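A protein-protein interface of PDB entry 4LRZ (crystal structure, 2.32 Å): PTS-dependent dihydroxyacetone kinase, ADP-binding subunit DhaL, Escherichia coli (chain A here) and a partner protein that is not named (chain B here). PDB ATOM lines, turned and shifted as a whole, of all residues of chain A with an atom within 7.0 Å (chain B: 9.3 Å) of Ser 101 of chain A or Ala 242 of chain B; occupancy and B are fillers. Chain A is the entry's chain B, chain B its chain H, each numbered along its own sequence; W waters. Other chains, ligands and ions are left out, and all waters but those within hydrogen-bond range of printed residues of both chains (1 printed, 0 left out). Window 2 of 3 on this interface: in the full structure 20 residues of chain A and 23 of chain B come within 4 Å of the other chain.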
ATOM      1  N   SER A   3      30.662 -11.833  25.705  1.00  0.00           N
ATOM      2  CA  SER A   3      31.283 -10.541  26.103  1.00  0.00           C
ATOM      3  C   SER A   3      31.613 -10.255  27.591  1.00  0.00           C
ATOM      4  O   SER A   3      31.061 -10.869  28.514  1.00  0.00           O
ATOM      5  CB  SER A   3      30.491  -9.367  25.509  1.00  0.00           C
ATOM      6  OG  SER A   3      29.309  -9.177  26.245  1.00  0.00           O
ATOM      7  N   LEU A   4      32.514  -9.288  27.786  1.00  0.00           N
ATOM      8  CA  LEU A   4      32.831  -8.745  29.113  1.00  0.00           C
ATOM      9  C   LEU A   4      32.072  -7.430  29.324  1.00  0.00           C
ATOM     10  O   LEU A   4      32.289  -6.476  28.595  1.00  0.00           O
ATOM     11  CB  LEU A   4      34.327  -8.503  29.244  1.00  0.00           C
ATOM     12  CG  LEU A   4      34.924  -8.437  30.650  1.00  0.00           C
ATOM     13  CD1 LEU A   4      34.867  -9.749  31.366  1.00  0.00           C
ATOM     14  CD2 LEU A   4      36.369  -7.991  30.519  1.00  0.00           C
ATOM     15  N   SER A   5      31.185  -7.395  30.319  1.00  0.00           N
ATOM     16  CA  SER A   5      30.425  -6.195  30.650  1.00  0.00           C
ATOM     17  C   SER A   5      31.272  -5.179  31.461  1.00  0.00           C
ATOM     18  O   SER A   5      32.326  -5.528  32.065  1.00  0.00           O
ATOM     19  CB  SER A   5      29.203  -6.590  31.462  1.00  0.00           C
ATOM     20  OG  SER A   5      29.652  -6.974  32.746  1.00  0.00           O
ATOM     21  N   ARG A   6      30.833  -3.922  31.506  1.00  0.00           N
ATOM     22  CA  ARG A   6      31.612  -3.004  32.335  1.00  0.00           C
ATOM     23  C   ARG A   6      31.477  -3.280  33.828  1.00  0.00           C
ATOM     24  O   ARG A   6      32.369  -2.961  34.572  1.00  0.00           O
ATOM     25  CB  ARG A   6      31.327  -1.538  32.044  1.00  0.00           C
ATOM     26  CG  ARG A   6      30.089  -1.050  32.625  1.00  0.00           C
ATOM     27  CD  ARG A   6      30.222  -0.366  33.987  1.00  0.00           C
ATOM     28  NE  ARG A   6      28.908  -0.391  34.626  1.00  0.00           N
ATOM     29  CZ  ARG A   6      27.738  -0.219  34.001  1.00  0.00           C
ATOM     30  NH1 ARG A   6      27.684   0.057  32.716  1.00  0.00           N
ATOM     31  NH2 ARG A   6      26.596  -0.288  34.671  1.00  0.00           N
ATOM     32  N   ILE A   9      34.152  -5.344  34.672  1.00  0.00           N
ATOM     33  CA  ILE A   9      35.437  -4.691  34.688  1.00  0.00           C
ATOM     34  C   ILE A   9      35.598  -4.062  36.075  1.00  0.00           C
ATOM     35  O   ILE A   9      36.642  -4.130  36.693  1.00  0.00           O
ATOM     36  CB  ILE A   9      35.606  -3.701  33.504  1.00  0.00           C
ATOM     37  CG1 ILE A   9      36.230  -4.447  32.332  1.00  0.00           C
ATOM     38  CG2 ILE A   9      36.582  -2.493  33.881  1.00  0.00           C
ATOM     39  CD1 ILE A   9      35.532  -4.258  31.057  1.00  0.00           C
ATOM     40  N   ILE A  62      33.382   1.940  30.334  1.00  0.00           N
ATOM     41  CA  ILE A  62      34.647   1.269  30.513  1.00  0.00           C
ATOM     42  C   ILE A  62      35.807   2.220  30.319  1.00  0.00           C
ATOM     43  O   ILE A  62      36.776   2.200  31.095  1.00  0.00           O
ATOM     44  CB  ILE A  62      34.756   0.036  29.585  1.00  0.00           C
ATOM     45  CG1 ILE A  62      33.700  -1.000  30.007  1.00  0.00           C
ATOM     46  CG2 ILE A  62      36.104  -0.617  29.698  1.00  0.00           C
ATOM     47  CD1 ILE A  62      33.492  -2.121  28.978  1.00  0.00           C
ATOM     48  N   ALA A  98      33.428   5.012  25.802  1.00  0.00           N
ATOM     49  CA  ALA A  98      31.975   4.808  25.695  1.00  0.00           C
ATOM     50  C   ALA A  98      31.483   3.360  25.741  1.00  0.00           C
ATOM     51  O   ALA A  98      30.299   3.153  25.870  1.00  0.00           O
ATOM     52  CB  ALA A  98      31.340   5.537  24.470  1.00  0.00           C
ATOM     53  N   ARG A  99      32.356   2.381  25.631  1.00  0.00           N
ATOM     54  CA  ARG A  99      31.932   0.942  25.721  1.00  0.00           C
ATOM     55  C   ARG A  99      31.190   0.566  26.978  1.00  0.00           C
ATOM     56  O   ARG A  99      31.466   1.062  28.040  1.00  0.00           O
ATOM     57  CB  ARG A  99      33.112  -0.001  25.574  1.00  0.00           C
ATOM     58  CG  ARG A  99      33.864   0.197  24.265  1.00  0.00           C
ATOM     59  CD  ARG A  99      33.300  -0.632  23.128  1.00  0.00           C
ATOM     60  NE  ARG A  99      34.151  -0.555  21.944  1.00  0.00           N
ATOM     61  CZ  ARG A  99      33.908  -1.211  20.820  1.00  0.00           C
ATOM     62  NH1 ARG A  99      32.839  -1.991  20.739  1.00  0.00           N
ATOM     63  NH2 ARG A  99      34.724  -1.082  19.777  1.00  0.00           N
ATOM     64  N   GLN A 100      30.238  -0.333  26.852  1.00  0.00           N
ATOM     65  CA  GLN A 100      29.624  -0.902  28.046  1.00  0.00           C
ATOM     66  C   GLN A 100      29.829  -2.395  28.069  1.00  0.00           C
ATOM     67  O   GLN A 100      29.348  -3.071  28.963  1.00  0.00           O
ATOM     68  CB  GLN A 100      28.135  -0.621  28.042  1.00  0.00           C
ATOM     69  CG  GLN A 100      27.633  -0.162  29.372  1.00  0.00           C
ATOM     70  CD  GLN A 100      27.276   1.277  29.343  1.00  0.00           C
ATOM     71  OE1 GLN A 100      28.011   2.102  29.852  1.00  0.00           O
ATOM     72  NE2 GLN A 100      26.139   1.605  28.730  1.00  0.00           N
ATOM     73  N   SER A 101      30.498  -2.914  27.046  1.00  0.00           N
ATOM     74  CA  SER A 101      30.733  -4.343  26.891  1.00  0.00           C
ATOM     75  C   SER A 101      31.784  -4.527  25.831  1.00  0.00           C
ATOM     76  O   SER A 101      31.893  -3.741  24.889  1.00  0.00           O
ATOM     77  CB  SER A 101      29.462  -5.097  26.442  1.00  0.00           C
ATOM     78  OG  SER A 101      29.385  -5.229  25.009  1.00  0.00           O
ATOM     79  N   LEU A 102      32.548  -5.585  25.967  1.00  0.00           N
ATOM     80  CA  LEU A 102      33.580  -5.864  25.010  1.00  0.00           C
ATOM     81  C   LEU A 102      33.477  -7.310  24.551  1.00  0.00           C
ATOM     82  O   LEU A 102      33.426  -8.236  25.384  1.00  0.00           O
ATOM     83  CB  LEU A 102      34.946  -5.607  25.652  1.00  0.00           C
ATOM     84  CG  LEU A 102      35.294  -4.177  26.115  1.00  0.00           C
ATOM     85  CD1 LEU A 102      36.642  -4.197  26.914  1.00  0.00           C
ATOM     86  CD2 LEU A 102      35.356  -3.186  24.965  1.00  0.00           C
ATOM     87  N   THR A 103      33.474  -7.512  23.235  1.00  0.00           N
ATOM     88  CA  THR A 103      33.657  -8.860  22.708  1.00  0.00           C
ATOM     89  C   THR A 103      35.090  -9.310  22.931  1.00  0.00           C
ATOM     90  O   THR A 103      35.967  -8.520  23.305  1.00  0.00           O
ATOM     91  CB  THR A 103      33.414  -8.938  21.216  1.00  0.00           C
ATOM     92  OG1 THR A 103      34.515  -8.305  20.538  1.00  0.00           O
ATOM     93  CG2 THR A 103      32.040  -8.338  20.848  1.00  0.00           C
ATOM     94  N   GLU A 106      37.636  -7.463  20.947  1.00  0.00           N
ATOM     95  CA  GLU A 106      37.819  -6.089  21.475  1.00  0.00           C
ATOM     96  C   GLU A 106      38.683  -6.109  22.727  1.00  0.00           C
ATOM     97  O   GLU A 106      39.565  -5.288  22.900  1.00  0.00           O
ATOM     98  CB  GLU A 106      36.444  -5.387  21.669  1.00  0.00           C
ATOM     99  CG  GLU A 106      35.734  -5.029  20.274  1.00  0.00           C
ATOM    100  CD  GLU A 106      34.212  -4.776  20.353  1.00  0.00           C
ATOM    101  OE1 GLU A 106      33.584  -5.033  21.401  1.00  0.00           O
ATOM    102  OE2 GLU A 106      33.601  -4.336  19.338  1.00  0.00           O
ATOM    103  N   LEU B 225      29.201   5.786  18.409  1.00  0.00           N
ATOM    104  CA  LEU B 225      28.083   6.067  19.291  1.00  0.00           C
ATOM    105  C   LEU B 225      28.602   6.345  20.689  1.00  0.00           C
ATOM    106  O   LEU B 225      29.392   5.566  21.243  1.00  0.00           O
ATOM    107  CB  LEU B 225      27.162   4.855  19.314  1.00  0.00           C
ATOM    108  CG  LEU B 225      25.855   5.133  20.020  1.00  0.00           C
ATOM    109  CD1 LEU B 225      24.880   5.437  18.933  1.00  0.00           C
ATOM    110  CD2 LEU B 225      25.362   3.960  20.772  1.00  0.00           C
ATOM    111  N   ILE B 228      23.110   6.324  23.983  1.00  0.00           N
ATOM    112  CA  ILE B 228      21.818   5.929  23.478  1.00  0.00           C
ATOM    113  C   ILE B 228      20.950   5.618  24.710  1.00  0.00           C
ATOM    114  O   ILE B 228      21.377   4.931  25.649  1.00  0.00           O
ATOM    115  CB  ILE B 228      21.921   4.720  22.524  1.00  0.00           C
ATOM    116  CG1 ILE B 228      20.558   4.367  21.920  1.00  0.00           C
ATOM    117  CG2 ILE B 228      22.500   3.498  23.261  1.00  0.00           C
ATOM    118  CD1 ILE B 228      20.656   3.408  20.777  1.00  0.00           C
ATOM    119  N   ALA B 233      16.698   2.931  21.916  1.00  0.00           N
ATOM    120  CA  ALA B 233      17.028   1.506  21.744  1.00  0.00           C
ATOM    121  C   ALA B 233      15.839   0.635  21.359  1.00  0.00           C
ATOM    122  O   ALA B 233      15.980  -0.219  20.487  1.00  0.00           O
ATOM    123  CB  ALA B 233      17.712   0.929  22.996  1.00  0.00           C
ATOM    124  N   LEU B 238      17.911  -1.425  18.570  1.00  0.00           N
ATOM    125  CA  LEU B 238      19.339  -1.629  18.842  1.00  0.00           C
ATOM    126  C   LEU B 238      19.578  -2.273  20.201  1.00  0.00           C
ATOM    127  O   LEU B 238      18.727  -2.230  21.095  1.00  0.00           O
ATOM    128  CB  LEU B 238      20.149  -0.324  18.718  1.00  0.00           C
ATOM    129  CG  LEU B 238      20.311   0.311  17.333  1.00  0.00           C
ATOM    130  CD1 LEU B 238      21.088   1.658  17.386  1.00  0.00           C
ATOM    131  CD2 LEU B 238      20.965  -0.672  16.344  1.00  0.00           C
ATOM    132  N   ASP B 239      20.743  -2.887  20.330  1.00  0.00           N
ATOM    133  CA  ASP B 239      21.169  -3.424  21.596  1.00  0.00           C
ATOM    134  C   ASP B 239      21.516  -2.293  22.550  1.00  0.00           C
ATOM    135  O   ASP B 239      22.454  -1.514  22.321  1.00  0.00           O
ATOM    136  CB  ASP B 239      22.359  -4.336  21.405  1.00  0.00           C
ATOM    137  CG  ASP B 239      22.897  -4.853  22.712  1.00  0.00           C
ATOM    138  OD1 ASP B 239      22.194  -4.770  23.750  1.00  0.00           O
ATOM    139  OD2 ASP B 239      24.036  -5.346  22.696  1.00  0.00           O
ATOM    140  N   ALA B 240      20.757  -2.228  23.635  1.00  0.00           N
ATOM    141  CA  ALA B 240      20.757  -1.067  24.512  1.00  0.00           C
ATOM    142  C   ALA B 240      22.085  -0.846  25.250  1.00  0.00           C
ATOM    143  O   ALA B 240      22.283   0.256  25.791  1.00  0.00           O
ATOM    144  CB  ALA B 240      19.574  -1.140  25.518  1.00  0.00           C
ATOM    145  N   THR B 241      22.967  -1.870  25.277  1.00  0.00           N
ATOM    146  CA  THR B 241      24.277  -1.781  25.958  1.00  0.00           C
ATOM    147  C   THR B 241      25.516  -2.242  25.157  1.00  0.00           C
ATOM    148  O   THR B 241      26.624  -2.040  25.623  1.00  0.00           O
ATOM    149  CB  THR B 241      24.318  -2.510  27.344  1.00  0.00           C
ATOM    150  OG1 THR B 241      24.596  -3.905  27.155  1.00  0.00           O
ATOM    151  CG2 THR B 241      23.024  -2.299  28.174  1.00  0.00           C
ATOM    152  N   ALA B 242      25.380  -2.879  23.995  1.00  0.00           N
ATOM    153  CA  ALA B 242      26.597  -3.119  23.183  1.00  0.00           C
ATOM    154  C   ALA B 242      26.730  -2.223  21.948  1.00  0.00           C
ATOM    155  O   ALA B 242      27.672  -2.384  21.142  1.00  0.00           O
ATOM    156  CB  ALA B 242      26.756  -4.560  22.810  1.00  0.00           C
ATOM    157  N   SER B 243      25.793  -1.283  21.804  1.00  0.00           N
ATOM    158  CA  SER B 243      25.859  -0.326  20.720  1.00  0.00           C
ATOM    159  C   SER B 243      26.884   0.775  20.988  1.00  0.00           C
ATOM    160  O   SER B 243      27.554   1.226  20.051  1.00  0.00           O
ATOM    161  CB  SER B 243      24.488   0.293  20.466  1.00  0.00           C
ATOM    162  OG  SER B 243      23.586  -0.702  20.035  1.00  0.00           O
ATOM    163  N   GLN B 244      27.016   1.196  22.253  1.00  0.00           N
ATOM    164  CA  GLN B 244      27.876   2.334  22.552  1.00  0.00           C
ATOM    165  C   GLN B 244      29.363   2.028  22.352  1.00  0.00           C
ATOM    166  O   GLN B 244      29.790   0.898  22.567  1.00  0.00           O
ATOM    167  CB  GLN B 244      27.520   3.051  23.857  1.00  0.00           C
ATOM    168  CG  GLN B 244      27.061   2.204  24.985  1.00  0.00           C
ATOM    169  CD  GLN B 244      25.593   1.806  24.916  1.00  0.00           C
ATOM    170  OE1 GLN B 244      24.745   2.362  25.619  1.00  0.00           O
ATOM    171  NE2 GLN B 244      25.307   0.792  24.127  1.00  0.00           N
ATOM    172  N   GLY B 245      30.111   3.010  21.842  1.00  0.00           N
ATOM    173  CA  GLY B 245      31.491   2.788  21.400  1.00  0.00           C
ATOM    174  C   GLY B 245      31.665   2.121  20.040  1.00  0.00           C
ATOM    175  O   GLY B 245      32.788   1.937  19.579  1.00  0.00           O
ATOM    176  N   ARG B 246      30.575   1.734  19.391  1.00  0.00           N
ATOM    177  CA  ARG B 246      30.664   1.157  18.024  1.00  0.00           C
ATOM    178  C   ARG B 246      30.277   2.149  16.919  1.00  0.00           C
ATOM    179  O   ARG B 246      29.501   3.106  17.159  1.00  0.00           O
ATOM    180  CB  ARG B 246      29.822  -0.114  17.897  1.00  0.00           C
ATOM    181  CG  ARG B 246      30.506  -1.342  18.509  1.00  0.00           C
ATOM    182  CD  ARG B 246      29.612  -2.587  18.518  1.00  0.00           C
ATOM    183  NE  ARG B 246      28.859  -2.779  17.273  1.00  0.00           N
ATOM    184  CZ  ARG B 246      29.320  -3.352  16.152  1.00  0.00           C
ATOM    185  NH1 ARG B 246      30.570  -3.786  16.068  1.00  0.00           N
ATOM    186  NH2 ARG B 246      28.523  -3.474  15.097  1.00  0.00           N
ATOM    187  N   ALA B 247      30.822   1.929  15.723  1.00  0.00           N
ATOM    188  CA  ALA B 247      30.485   2.769  14.574  1.00  0.00           C
ATOM    189  C   ALA B 247      28.978   2.755  14.330  1.00  0.00           C
ATOM    190  O   ALA B 247      28.367   1.694  14.255  1.00  0.00           O
ATOM    191  CB  ALA B 247      31.242   2.313  13.314  1.00  0.00           C
ATOM    192  N   GLU B 250      27.927   0.761  11.257  1.00  0.00           N
ATOM    193  CA  GLU B 250      27.781  -0.677  11.532  1.00  0.00           C
ATOM    194  C   GLU B 250      26.480  -1.023  12.265  1.00  0.00           C
ATOM    195  O   GLU B 250      26.034  -2.170  12.238  1.00  0.00           O
ATOM    196  CB  GLU B 250      28.970  -1.209  12.342  1.00  0.00           C
ATOM    197  CG  GLU B 250      30.201  -1.512  11.513  1.00  0.00           C
ATOM    198  CD  GLU B 250      31.492  -1.428  12.323  1.00  0.00           C
ATOM    199  OE1 GLU B 250      31.546  -1.926  13.486  1.00  0.00           O
ATOM    200  OE2 GLU B 250      32.466  -0.856  11.782  1.00  0.00           O
ATOM    201  N   LEU B 251      25.870  -0.042  12.915  1.00  0.00           N
ATOM    202  CA  LEU B 251      24.740  -0.330  13.778  1.00  0.00           C
ATOM    203  C   LEU B 251      23.402  -0.242  13.072  1.00  0.00           C
ATOM    204  O   LEU B 251      22.539  -1.089  13.278  1.00  0.00           O
ATOM    205  CB  LEU B 251      24.764   0.566  15.016  1.00  0.00           C
ATOM    206  CG  LEU B 251      25.922   0.249  15.984  1.00  0.00           C
ATOM    207  CD1 LEU B 251      25.959   1.248  17.114  1.00  0.00           C
ATOM    208  CD2 LEU B 251      25.858  -1.184  16.530  1.00  0.00           C
HETATM  209  O   HOH W   1      28.774  -1.000  24.649  1.00  0.00           O
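Printed residues of chain B within 4 Å of Arg 99 of chain A: Gln 244, Gly 245 and Arg 246. Of the printed residues of chain B, Gln 100 of chain A touches Thr 241 and Gln 244. Printed residues of chain B within 4 Å of Ser 101 of chain A: Ala 242. Of chain A, only Ser 101 comes within 4 Å of Ala 242 of chain B. Of the printed residues of chain A, Gly 245 of chain B touches Ala 98 (3.8 Å) and Arg 99 (3.6 Å). The nearest residue of chain B that does not touch Ser 101 of chain A is Thr 241 of chain B (4.2 Å).
Ala 98 of chain A touches Leu 225 of chain B (CB to O, 3.8 Å). Gln 244 of chain B touches Ala 98 of chain A. Ala 98 of chain A touches Gly 245 of chain B. Arg 99 of chain A touches Gln 244 of chain B. Arg 99 of chain A touches Gly 245 of chain B. CG of Arg 246 of chain B touches NH1 of Arg 99 of chain A (3.3 Å). O of Thr 241 of chain B touches CB of Gln 100 of chain A, at 3.2 Å. Ser 101 of chain A touches Ala 242 of chain B (OG to CB, 3.5 Å).
OE1 of Gln 244 of chain B is in hydrogen-bond range of NE2 of Gln 100 of chain A (3.5 Å).
Water W1 lies within hydrogen-bond range of O of Thr 241 of chain B (2.6 Å), N of Gln 100 of chain A (2.7 Å) and O of Gln 244 of chain B (3.0 Å).
Of the 13 printed residues of chain A, 4 touch a printed residue of chain B. Hydrophobic or aromatic side chains of chain A that line the printed part of chain B: Ala 98. Along chain A the printed residues that touch a printed residue of chain B span positions 98 to 101. Of the 15 printed residues of chain B, 6 touch a printed residue of chain A. Among the printed residues, 9 pairs touch across the chains. Among the printed residues, no Asp or Glu carboxylate lies within 4 Å of a Lys or Arg side-chain nitrogen of the other chain.
The backbone NH (N) of Arg 6 of chain A is in hydrogen-bond range of the backbone carbonyl oxygen (O) of Gln 100 of chain A (3.1 Å). The guanidinium group of Arg 99 of chain A is in salt-bridge range of the side-chain carboxylate of Glu 106 of chain A, 2.8 Å away. O of Arg 246 of chain B lies within hydrogen-bond range of N of Leu 225 of chain B, 3.0 Å away. The backbone NH (N) of Thr 241 of chain B sits close to the side-chain carboxylate (OD1) of Asp 239 of chain B (3.4 Å). OD2 of Asp 239 of chain B sits close to N of Ala 242 of chain B (3.1 Å). The guanidinium group (NH1) of Arg 246 of chain B is in salt-bridge range of the side-chain carboxylate (OE1) of Glu 250 of chain B (3.3 Å).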
